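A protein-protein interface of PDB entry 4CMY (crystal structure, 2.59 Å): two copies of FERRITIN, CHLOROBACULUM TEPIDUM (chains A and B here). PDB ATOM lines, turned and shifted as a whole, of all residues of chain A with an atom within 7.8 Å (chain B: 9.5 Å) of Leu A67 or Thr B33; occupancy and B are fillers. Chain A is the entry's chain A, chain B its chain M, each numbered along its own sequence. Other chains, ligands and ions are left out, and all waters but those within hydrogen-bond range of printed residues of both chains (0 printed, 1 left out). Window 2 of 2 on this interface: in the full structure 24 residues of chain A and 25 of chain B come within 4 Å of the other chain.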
ATOM      1  N   LEU A   2       1.065  30.226 -16.343  1.00  0.00           N
ATOM      2  CA  LEU A   2       1.040  29.158 -17.380  1.00  0.00           C
ATOM      3  C   LEU A   2       0.463  29.662 -18.688  1.00  0.00           C
ATOM      4  O   LEU A   2      -0.555  30.305 -18.704  1.00  0.00           O
ATOM      5  CB  LEU A   2       0.229  27.937 -16.927  1.00  0.00           C
ATOM      6  CG  LEU A   2       0.852  26.984 -15.907  1.00  0.00           C
ATOM      7  CD1 LEU A   2      -0.171  25.941 -15.511  1.00  0.00           C
ATOM      8  CD2 LEU A   2       2.068  26.304 -16.468  1.00  0.00           C
ATOM      9  N   LEU A   7      -1.463  24.950 -20.171  1.00  0.00           N
ATOM     10  CA  LEU A   7      -2.600  24.762 -19.265  1.00  0.00           C
ATOM     11  C   LEU A   7      -3.588  23.772 -19.846  1.00  0.00           C
ATOM     12  O   LEU A   7      -4.012  22.847 -19.162  1.00  0.00           O
ATOM     13  CB  LEU A   7      -3.361  26.050 -19.045  1.00  0.00           C
ATOM     14  CG  LEU A   7      -4.057  26.304 -17.717  1.00  0.00           C
ATOM     15  CD1 LEU A   7      -5.286  27.175 -17.922  1.00  0.00           C
ATOM     16  CD2 LEU A   7      -4.431  25.048 -16.955  1.00  0.00           C
ATOM     17  N   ASN A  11      -4.383  20.189 -18.033  1.00  0.00           N
ATOM     18  CA  ASN A  11      -5.767  19.798 -17.727  1.00  0.00           C
ATOM     19  C   ASN A  11      -6.233  18.582 -18.494  1.00  0.00           C
ATOM     20  O   ASN A  11      -7.024  17.790 -18.000  1.00  0.00           O
ATOM     21  CB  ASN A  11      -6.715  20.970 -17.953  1.00  0.00           C
ATOM     22  CG  ASN A  11      -6.761  21.897 -16.767  1.00  0.00           C
ATOM     23  OD1 ASN A  11      -6.581  21.471 -15.631  1.00  0.00           O
ATOM     24  ND2 ASN A  11      -7.056  23.151 -17.008  1.00  0.00           N
ATOM     25  N   PHE A  58      -3.030  18.168 -10.649  1.00  0.00           N
ATOM     26  CA  PHE A  58      -4.063  19.054 -10.182  1.00  0.00           C
ATOM     27  C   PHE A  58      -3.455  20.098  -9.257  1.00  0.00           C
ATOM     28  O   PHE A  58      -3.688  21.296  -9.412  1.00  0.00           O
ATOM     29  CB  PHE A  58      -5.099  18.202  -9.492  1.00  0.00           C
ATOM     30  CG  PHE A  58      -6.215  18.951  -8.841  1.00  0.00           C
ATOM     31  CD1 PHE A  58      -6.130  19.319  -7.511  1.00  0.00           C
ATOM     32  CD2 PHE A  58      -7.398  19.157  -9.495  1.00  0.00           C
ATOM     33  CE1 PHE A  58      -7.189  19.941  -6.875  1.00  0.00           C
ATOM     34  CE2 PHE A  58      -8.462  19.773  -8.873  1.00  0.00           C
ATOM     35  CZ  PHE A  58      -8.363  20.160  -7.561  1.00  0.00           C
ATOM     36  N   ILE A  61      -1.010  22.613 -11.159  1.00  0.00           N
ATOM     37  CA  ILE A  61      -1.765  23.618 -11.907  1.00  0.00           C
ATOM     38  C   ILE A  61      -2.263  24.707 -10.947  1.00  0.00           C
ATOM     39  O   ILE A  61      -2.044  25.885 -11.191  1.00  0.00           O
ATOM     40  CB  ILE A  61      -2.953  22.992 -12.648  1.00  0.00           C
ATOM     41  CG1 ILE A  61      -2.462  22.073 -13.751  1.00  0.00           C
ATOM     42  CG2 ILE A  61      -3.809  24.059 -13.259  1.00  0.00           C
ATOM     43  CD1 ILE A  61      -3.485  21.051 -14.147  1.00  0.00           C
ATOM     44  N   ASN A  62      -2.901  24.303  -9.859  1.00  0.00           N
ATOM     45  CA  ASN A  62      -3.454  25.268  -8.903  1.00  0.00           C
ATOM     46  C   ASN A  62      -2.380  26.112  -8.253  1.00  0.00           C
ATOM     47  O   ASN A  62      -2.570  27.303  -8.083  1.00  0.00           O
ATOM     48  CB  ASN A  62      -4.310  24.579  -7.838  1.00  0.00           C
ATOM     49  CG  ASN A  62      -5.567  23.977  -8.414  1.00  0.00           C
ATOM     50  OD1 ASN A  62      -6.107  24.459  -9.424  1.00  0.00           O
ATOM     51  ND2 ASN A  62      -6.046  22.922  -7.802  1.00  0.00           N
ATOM     52  N   GLU A  63      -1.229  25.514  -7.936  1.00  0.00           N
ATOM     53  CA  GLU A  63      -0.109  26.260  -7.341  1.00  0.00           C
ATOM     54  C   GLU A  63       0.411  27.353  -8.291  1.00  0.00           C
ATOM     55  O   GLU A  63       0.824  28.403  -7.817  1.00  0.00           O
ATOM     56  CB  GLU A  63       1.040  25.343  -6.930  1.00  0.00           C
ATOM     57  CG  GLU A  63       0.743  24.507  -5.696  1.00  0.00           C
ATOM     58  CD  GLU A  63       1.756  23.385  -5.444  1.00  0.00           C
ATOM     59  OE1 GLU A  63       2.831  23.369  -6.107  1.00  0.00           O
ATOM     60  OE2 GLU A  63       1.450  22.502  -4.597  1.00  0.00           O
ATOM     61  N   THR A  64       0.368  27.121  -9.609  1.00  0.00           N
ATOM     62  CA  THR A  64       0.819  28.143 -10.549  1.00  0.00           C
ATOM     63  C   THR A  64      -0.160  29.318 -10.662  1.00  0.00           C
ATOM     64  O   THR A  64       0.137  30.298 -11.335  1.00  0.00           O
ATOM     65  CB  THR A  64       0.998  27.618 -11.978  1.00  0.00           C
ATOM     66  OG1 THR A  64      -0.260  27.272 -12.552  1.00  0.00           O
ATOM     67  CG2 THR A  64       1.936  26.446 -12.028  1.00  0.00           C
ATOM     68  N   GLY A  65      -1.338  29.197 -10.045  1.00  0.00           N
ATOM     69  CA  GLY A  65      -2.362  30.233 -10.110  1.00  0.00           C
ATOM     70  C   GLY A  65      -3.450  30.040 -11.141  1.00  0.00           C
ATOM     71  O   GLY A  65      -4.318  30.864 -11.245  1.00  0.00           O
ATOM     72  N   SER A  66      -3.399  28.968 -11.913  1.00  0.00           N
ATOM     73  CA  SER A  66      -4.477  28.631 -12.831  1.00  0.00           C
ATOM     74  C   SER A  66      -5.457  27.692 -12.160  1.00  0.00           C
ATOM     75  O   SER A  66      -5.229  27.227 -11.063  1.00  0.00           O
ATOM     76  CB  SER A  66      -3.929  27.970 -14.098  1.00  0.00           C
ATOM     77  OG  SER A  66      -3.035  28.824 -14.772  1.00  0.00           O
ATOM     78  N   LEU A  67      -6.568  27.440 -12.832  1.00  0.00           N
ATOM     79  CA  LEU A  67      -7.637  26.647 -12.297  1.00  0.00           C
ATOM     80  C   LEU A  67      -7.645  25.265 -12.951  1.00  0.00           C
ATOM     81  O   LEU A  67      -7.850  25.152 -14.155  1.00  0.00           O
ATOM     82  CB  LEU A  67      -8.948  27.351 -12.522  1.00  0.00           C
ATOM     83  CG  LEU A  67     -10.228  26.583 -12.184  1.00  0.00           C
ATOM     84  CD1 LEU A  67     -10.410  26.430 -10.684  1.00  0.00           C
ATOM     85  CD2 LEU A  67     -11.409  27.330 -12.768  1.00  0.00           C
ATOM     86  N   ALA A  68      -7.405  24.212 -12.156  1.00  0.00           N
ATOM     87  CA  ALA A  68      -7.380  22.883 -12.689  1.00  0.00           C
ATOM     88  C   ALA A  68      -8.787  22.465 -12.964  1.00  0.00           C
ATOM     89  O   ALA A  68      -9.721  22.825 -12.242  1.00  0.00           O
ATOM     90  CB  ALA A  68      -6.737  21.946 -11.712  1.00  0.00           C
ATOM     91  N   LEU A  69      -8.958  21.705 -14.037  1.00  0.00           N
ATOM     92  CA  LEU A  69     -10.273  21.264 -14.462  1.00  0.00           C
ATOM     93  C   LEU A  69     -10.275  19.745 -14.600  1.00  0.00           C
ATOM     94  O   LEU A  69      -9.437  19.189 -15.283  1.00  0.00           O
ATOM     95  CB  LEU A  69     -10.617  21.883 -15.812  1.00  0.00           C
ATOM     96  CG  LEU A  69     -10.774  23.394 -15.849  1.00  0.00           C
ATOM     97  CD1 LEU A  69     -10.905  23.909 -17.272  1.00  0.00           C
ATOM     98  CD2 LEU A  69     -11.989  23.811 -15.014  1.00  0.00           C
ATOM     99  N   ILE A  70     -11.281  19.094 -14.022  1.00  0.00           N
ATOM    100  CA  ILE A  70     -11.407  17.654 -14.091  1.00  0.00           C
ATOM    101  C   ILE A  70     -11.990  17.211 -15.425  1.00  0.00           C
ATOM    102  O   ILE A  70     -11.551  16.210 -15.984  1.00  0.00           O
ATOM    103  CB  ILE A  70     -12.330  17.115 -12.974  1.00  0.00           C
ATOM    104  CG1 ILE A  70     -11.953  17.691 -11.600  1.00  0.00           C
ATOM    105  CG2 ILE A  70     -12.256  15.593 -12.920  1.00  0.00           C
ATOM    106  CD1 ILE A  70     -10.623  17.201 -11.054  1.00  0.00           C
ATOM    107  N   LEU B  25     -13.661  17.970  -5.780  1.00  0.00           N
ATOM    108  CA  LEU B  25     -12.329  18.346  -6.263  1.00  0.00           C
ATOM    109  C   LEU B  25     -12.413  19.640  -7.027  1.00  0.00           C
ATOM    110  O   LEU B  25     -11.615  20.547  -6.819  1.00  0.00           O
ATOM    111  CB  LEU B  25     -11.766  17.268  -7.179  1.00  0.00           C
ATOM    112  CG  LEU B  25     -10.620  16.398  -6.695  1.00  0.00           C
ATOM    113  CD1 LEU B  25     -10.384  16.393  -5.206  1.00  0.00           C
ATOM    114  CD2 LEU B  25     -10.850  14.969  -7.174  1.00  0.00           C
ATOM    115  N   GLN B  26     -13.393  19.743  -7.921  1.00  0.00           N
ATOM    116  CA  GLN B  26     -13.530  20.943  -8.743  1.00  0.00           C
ATOM    117  C   GLN B  26     -13.822  22.171  -7.884  1.00  0.00           C
ATOM    118  O   GLN B  26     -13.302  23.255  -8.143  1.00  0.00           O
ATOM    119  CB  GLN B  26     -14.600  20.741  -9.801  1.00  0.00           C
ATOM    120  CG  GLN B  26     -14.616  21.814 -10.881  1.00  0.00           C
ATOM    121  CD  GLN B  26     -13.331  21.877 -11.658  1.00  0.00           C
ATOM    122  OE1 GLN B  26     -13.145  21.164 -12.647  1.00  0.00           O
ATOM    123  NE2 GLN B  26     -12.433  22.744 -11.222  1.00  0.00           N
ATOM    124  N   MET B  27     -14.649  21.996  -6.852  1.00  0.00           N
ATOM    125  CA  MET B  27     -14.963  23.086  -5.932  1.00  0.00           C
ATOM    126  C   MET B  27     -13.696  23.502  -5.230  1.00  0.00           C
ATOM    127  O   MET B  27     -13.444  24.687  -5.048  1.00  0.00           O
ATOM    128  CB  MET B  27     -16.030  22.673  -4.925  1.00  0.00           C
ATOM    129  CG  MET B  27     -17.438  22.585  -5.487  1.00  0.00           C
ATOM    130  SD  MET B  27     -18.633  21.993  -4.258  1.00  0.00           S
ATOM    131  CE  MET B  27     -20.169  22.231  -5.146  1.00  0.00           C
ATOM    132  N   SER B  28     -12.891  22.528  -4.827  1.00  0.00           N
ATOM    133  CA  SER B  28     -11.646  22.819  -4.146  1.00  0.00           C
ATOM    134  C   SER B  28     -10.768  23.718  -5.000  1.00  0.00           C
ATOM    135  O   SER B  28     -10.187  24.682  -4.494  1.00  0.00           O
ATOM    136  CB  SER B  28     -10.896  21.525  -3.832  1.00  0.00           C
ATOM    137  OG  SER B  28      -9.733  21.800  -3.077  1.00  0.00           O
ATOM    138  N   ALA B  29     -10.662  23.385  -6.280  1.00  0.00           N
ATOM    139  CA  ALA B  29      -9.806  24.142  -7.195  1.00  0.00           C
ATOM    140  C   ALA B  29     -10.301  25.562  -7.322  1.00  0.00           C
ATOM    141  O   ALA B  29      -9.491  26.506  -7.309  1.00  0.00           O
ATOM    142  CB  ALA B  29      -9.771  23.490  -8.548  1.00  0.00           C
ATOM    143  N   TRP B  30     -11.619  25.741  -7.422  1.00  0.00           N
ATOM    144  CA  TRP B  30     -12.188  27.083  -7.526  1.00  0.00           C
ATOM    145  C   TRP B  30     -11.889  27.902  -6.260  1.00  0.00           C
ATOM    146  O   TRP B  30     -11.488  29.070  -6.332  1.00  0.00           O
ATOM    147  CB  TRP B  30     -13.703  27.022  -7.774  1.00  0.00           C
ATOM    148  CG  TRP B  30     -14.313  28.355  -7.931  1.00  0.00           C
ATOM    149  CD1 TRP B  30     -14.332  29.121  -9.068  1.00  0.00           C
ATOM    150  CD2 TRP B  30     -14.925  29.147  -6.909  1.00  0.00           C
ATOM    151  NE1 TRP B  30     -14.935  30.324  -8.808  1.00  0.00           N
ATOM    152  CE2 TRP B  30     -15.319  30.375  -7.498  1.00  0.00           C
ATOM    153  CE3 TRP B  30     -15.200  28.940  -5.578  1.00  0.00           C
ATOM    154  CZ2 TRP B  30     -15.978  31.398  -6.775  1.00  0.00           C
ATOM    155  CZ3 TRP B  30     -15.858  29.961  -4.859  1.00  0.00           C
ATOM    156  CH2 TRP B  30     -16.217  31.167  -5.466  1.00  0.00           C
ATOM    157  N   LEU B  31     -12.093  27.278  -5.103  1.00  0.00           N
ATOM    158  CA  LEU B  31     -11.885  27.945  -3.832  1.00  0.00           C
ATOM    159  C   LEU B  31     -10.464  28.441  -3.677  1.00  0.00           C
ATOM    160  O   LEU B  31     -10.251  29.496  -3.124  1.00  0.00           O
ATOM    161  CB  LEU B  31     -12.259  27.004  -2.692  1.00  0.00           C
ATOM    162  CG  LEU B  31     -13.765  26.745  -2.578  1.00  0.00           C
ATOM    163  CD1 LEU B  31     -14.063  25.498  -1.758  1.00  0.00           C
ATOM    164  CD2 LEU B  31     -14.439  27.948  -1.936  1.00  0.00           C
ATOM    165  N   LEU B  32      -9.484  27.689  -4.188  1.00  0.00           N
ATOM    166  CA  LEU B  32      -8.103  28.154  -4.167  1.00  0.00           C
ATOM    167  C   LEU B  32      -7.919  29.427  -4.978  1.00  0.00           C
ATOM    168  O   LEU B  32      -7.205  30.317  -4.532  1.00  0.00           O
ATOM    169  CB  LEU B  32      -7.131  27.099  -4.662  1.00  0.00           C
ATOM    170  CG  LEU B  32      -6.945  25.908  -3.706  1.00  0.00           C
ATOM    171  CD1 LEU B  32      -6.216  24.772  -4.389  1.00  0.00           C
ATOM    172  CD2 LEU B  32      -6.209  26.309  -2.453  1.00  0.00           C
ATOM    173  N   THR B  33      -8.626  29.596  -6.089  1.00  0.00           N
ATOM    174  CA  THR B  33      -8.554  30.893  -6.824  1.00  0.00           C
ATOM    175  C   THR B  33      -9.141  32.084  -6.044  1.00  0.00           C
ATOM    176  O   THR B  33      -8.817  33.210  -6.363  1.00  0.00           O
ATOM    177  CB  THR B  33      -9.250  30.869  -8.209  1.00  0.00           C
ATOM    178  OG1 THR B  33     -10.684  30.871  -8.060  1.00  0.00           O
ATOM    179  CG2 THR B  33      -8.802  29.646  -9.024  1.00  0.00           C
ATOM    180  N   GLN B  34      -9.967  31.829  -5.031  1.00  0.00           N
ATOM    181  CA  GLN B  34     -10.508  32.876  -4.138  1.00  0.00           C
ATOM    182  C   GLN B  34      -9.686  33.041  -2.875  1.00  0.00           C
ATOM    183  O   GLN B  34     -10.049  33.841  -2.014  1.00  0.00           O
ATOM    184  CB  GLN B  34     -11.924  32.514  -3.693  1.00  0.00           C
ATOM    185  CG  GLN B  34     -12.859  32.163  -4.822  1.00  0.00           C
ATOM    186  CD  GLN B  34     -12.941  33.170  -5.916  1.00  0.00           C
ATOM    187  OE1 GLN B  34     -12.580  32.716  -6.919  1.00  0.00           O
ATOM    188  NE2 GLN B  34     -13.325  34.450  -5.779  1.00  0.00           N
ATOM    189  N   SER B  35      -8.566  32.314  -2.767  1.00  0.00           N
ATOM    190  CA  SER B  35      -7.723  32.285  -1.539  1.00  0.00           C
ATOM    191  C   SER B  35      -8.448  31.772  -0.296  1.00  0.00           C
ATOM    192  O   SER B  35      -8.102  32.145   0.810  1.00  0.00           O
ATOM    193  CB  SER B  35      -7.098  33.661  -1.257  1.00  0.00           C
ATOM    194  OG  SER B  35      -5.945  33.830  -2.044  1.00  0.00           O
ATOM    195  N   LEU B  36      -9.471  30.945  -0.497  1.00  0.00           N
ATOM    196  CA  LEU B  36     -10.151  30.300   0.583  1.00  0.00           C
ATOM    197  C   LEU B  36      -9.506  28.934   0.811  1.00  0.00           C
ATOM    198  O   LEU B  36     -10.107  27.887   0.573  1.00  0.00           O
ATOM    199  CB  LEU B  36     -11.640  30.175   0.260  1.00  0.00           C
ATOM    200  CG  LEU B  36     -12.377  31.519   0.184  1.00  0.00           C
ATOM    201  CD1 LEU B  36     -13.750  31.391  -0.480  1.00  0.00           C
ATOM    202  CD2 LEU B  36     -12.534  32.085   1.581  1.00  0.00           C
ATOM    203  N   ASP B  37      -8.283  28.951   1.315  1.00  0.00           N
ATOM    204  CA  ASP B  37      -7.431  27.765   1.408  1.00  0.00           C
ATOM    205  C   ASP B  37      -7.949  26.644   2.347  1.00  0.00           C
ATOM    206  O   ASP B  37      -7.860  25.469   2.006  1.00  0.00           O
ATOM    207  CB  ASP B  37      -6.018  28.193   1.804  1.00  0.00           C
ATOM    208  CG  ASP B  37      -5.299  28.981   0.681  1.00  0.00           C
ATOM    209  OD1 ASP B  37      -5.913  29.249  -0.392  1.00  0.00           O
ATOM    210  OD2 ASP B  37      -4.087  29.305   0.862  1.00  0.00           O
ATOM    211  N   ALA B  40     -10.996  25.117   0.689  1.00  0.00           N
ATOM    212  CA  ALA B  40     -10.463  24.266  -0.369  1.00  0.00           C
ATOM    213  C   ALA B  40      -9.980  22.929   0.178  1.00  0.00           C
ATOM    214  O   ALA B  40     -10.177  21.892  -0.442  1.00  0.00           O
ATOM    215  CB  ALA B  40      -9.331  24.954  -1.101  1.00  0.00           C
ATOM    216  N   PRO B  76     -19.094  19.803 -14.486  1.00  0.00           N
ATOM    217  CA  PRO B  76     -19.121  21.098 -15.176  1.00  0.00           C
ATOM    218  C   PRO B  76     -18.011  21.986 -14.624  1.00  0.00           C
ATOM    219  O   PRO B  76     -17.641  21.841 -13.450  1.00  0.00           O
ATOM    220  CB  PRO B  76     -20.519  21.657 -14.846  1.00  0.00           C
ATOM    221  CG  PRO B  76     -20.903  20.982 -13.566  1.00  0.00           C
ATOM    222  CD  PRO B  76     -20.256  19.622 -13.589  1.00  0.00           C
ATOM    223  N   ALA B  77     -17.477  22.858 -15.488  1.00  0.00           N
ATOM    224  CA  ALA B  77     -16.512  23.877 -15.080  1.00  0.00           C
ATOM    225  C   ALA B  77     -17.150  24.748 -13.996  1.00  0.00           C
ATOM    226  O   ALA B  77     -18.370  24.752 -13.825  1.00  0.00           O
ATOM    227  CB  ALA B  77     -16.069  24.719 -16.273  1.00  0.00           C
ATOM    228  N   PRO B  78     -16.346  25.451 -13.234  1.00  0.00           N
ATOM    229  CA  PRO B  78     -16.900  26.185 -12.104  1.00  0.00           C
ATOM    230  C   PRO B  78     -17.702  27.396 -12.509  1.00  0.00           C
ATOM    231  O   PRO B  78     -17.130  28.388 -12.929  1.00  0.00           O
ATOM    232  CB  PRO B  78     -15.648  26.635 -11.351  1.00  0.00           C
ATOM    233  CG  PRO B  78     -14.669  25.553 -11.631  1.00  0.00           C
ATOM    234  CD  PRO B  78     -14.909  25.234 -13.084  1.00  0.00           C
ATOM    235  N   GLU B  79     -19.014  27.338 -12.315  1.00  0.00           N
ATOM    236  CA  GLU B  79     -19.852  28.503 -12.548  1.00  0.00           C
ATOM    237  C   GLU B  79     -19.799  29.537 -11.366  1.00  0.00           C
ATOM    238  O   GLU B  79     -20.065  30.711 -11.573  1.00  0.00           O
ATOM    239  CB  GLU B  79     -21.291  28.054 -12.819  1.00  0.00           C
ATOM    240  N   TRP B  80     -19.432  29.111 -10.157  1.00  0.00           N
ATOM    241  CA  TRP B  80     -19.855  29.800  -8.928  1.00  0.00           C
ATOM    242  C   TRP B  80     -19.426  31.241  -8.861  1.00  0.00           C
ATOM    243  O   TRP B  80     -18.292  31.560  -9.096  1.00  0.00           O
ATOM    244  CB  TRP B  80     -19.414  29.014  -7.657  1.00  0.00           C
ATOM    245  CG  TRP B  80     -19.841  27.567  -7.744  1.00  0.00           C
ATOM    246  CD1 TRP B  80     -21.117  27.059  -7.633  1.00  0.00           C
ATOM    247  CD2 TRP B  80     -18.994  26.471  -8.052  1.00  0.00           C
ATOM    248  NE1 TRP B  80     -21.090  25.699  -7.834  1.00  0.00           N
ATOM    249  CE2 TRP B  80     -19.791  25.322  -8.091  1.00  0.00           C
ATOM    250  CE3 TRP B  80     -17.617  26.353  -8.286  1.00  0.00           C
ATOM    251  CZ2 TRP B  80     -19.264  24.066  -8.359  1.00  0.00           C
ATOM    252  CZ3 TRP B  80     -17.084  25.092  -8.565  1.00  0.00           C
ATOM    253  CH2 TRP B  80     -17.905  23.967  -8.601  1.00  0.00           C
ATOM    254  N   LYS B  81     -20.367  32.098  -8.477  1.00  0.00           N
ATOM    255  CA  LYS B  81     -20.143  33.544  -8.355  1.00  0.00           C
ATOM    256  C   LYS B  81     -19.658  33.918  -6.936  1.00  0.00           C
ATOM    257  O   LYS B  81     -18.988  34.918  -6.767  1.00  0.00           O
ATOM    258  CB  LYS B  81     -21.426  34.319  -8.726  1.00  0.00           C
ATOM    259  N   LEU B  86     -21.554  28.319  -3.911  1.00  0.00           N
ATOM    260  CA  LEU B  86     -20.899  26.990  -3.950  1.00  0.00           C
ATOM    261  C   LEU B  86     -21.369  26.119  -2.798  1.00  0.00           C
ATOM    262  O   LEU B  86     -21.705  24.945  -2.996  1.00  0.00           O
ATOM    263  CB  LEU B  86     -19.395  27.159  -4.019  1.00  0.00           C
ATOM    264  CG  LEU B  86     -18.247  26.351  -3.399  1.00  0.00           C
ATOM    265  CD1 LEU B  86     -18.613  25.039  -2.748  1.00  0.00           C
ATOM    266  CD2 LEU B  86     -17.174  26.125  -4.444  1.00  0.00           C
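The backbone carbonyl oxygen (O) of Ala A68 is in hydrogen-bond range of the side-chain amide nitrogen (NE2) of Gln B26 (2.9 Å). OE1 of Gln B26 sits at hydrogen-bond distance from N of Ile A70 (3.1 Å).
O of Leu B25 touches CZ of Phe A58, 3.4 Å away. Phe A58 touches Ala B29. ND2 of Asn A62 touches CB of Ala B29, at 3.8 Å. Asn A62 touches Leu B32. Ala B29 touches Leu A67. CD1 of Leu A67 touches N of Trp B30, at 3.5 Å. Leu A67 touches Thr B33 (CD1 to CG2, 3.96 Å). Pro B78 touches Leu A67. Gln B26 touches Leu A69. Leu A69 touches Pro B78.
Ser A66 touches none of the printed residues of chain B. Of chain B, only Ala B29 (3.5 Å), Trp B30 (3.5 Å), Thr B33 (3.96 Å) and Pro B78 (3.9 Å) come within 4 Å of Leu A67. Ala A68 touches two residues of chain B. Printed residues of chain B within 4 Å of Leu A69: Gln B26 and Pro B78. Printed residues of chain B within 4 Å of Ile A70: Gln B26. Of the printed residues of chain A, Ala B29 touches Phe A58, Asn A62, Leu A67 and Ala A68. Leu B31 touches none of the printed residues of chain A. Thr B33 touches just one residue of chain A: Leu A67 (3.96 Å). Of the printed residues of chain A, Pro B78 touches Leu A67 and Leu A69. The nearest residue of chain A that does not touch Thr B33 is Ser A66 (4.8 Å).
The backbone NH (N) of Leu A69 is in hydrogen-bond range of the side-chain amide oxygen (OD1) of Asn A11, 2.9 Å away. The backbone carbonyl oxygen of Phe A58 lies within hydrogen-bond range of the side-chain amide nitrogen of Asn A62, 3.3 Å away. The side-chain amide oxygen (OD1) of Asn A62 sits close to the backbone carbonyl oxygen (O) of Ser A66 (3.3 Å). The backbone NH of Ala A68 lies within hydrogen-bond range of the side-chain amide oxygen of Asn A62 (3.0 Å). The backbone carbonyl oxygen of Trp B30 is in hydrogen-bond range of the side-chain hydroxyl of Thr B33 (2.6 Å). The side-chain amide oxygen (OE1) of Gln B34 is in hydrogen-bond range of the side-chain hydroxyl (OG1) of Thr B33 (2.9 Å).
No position is printed for both chains.
Of the 21 printed residues of chain B, 7 touch a printed residue of chain A. Hydrophobic or aromatic side chains of chain A within 4 Å of the printed part of chain B: Phe A58, Leu A67, Leu A69 and Ile A70. Among the printed residues, 13 pairs touch across the chains. Among the printed residues, no Asp or Glu carboxylate lies within 4 Å of a Lys or Arg side-chain nitrogen of the other chain.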
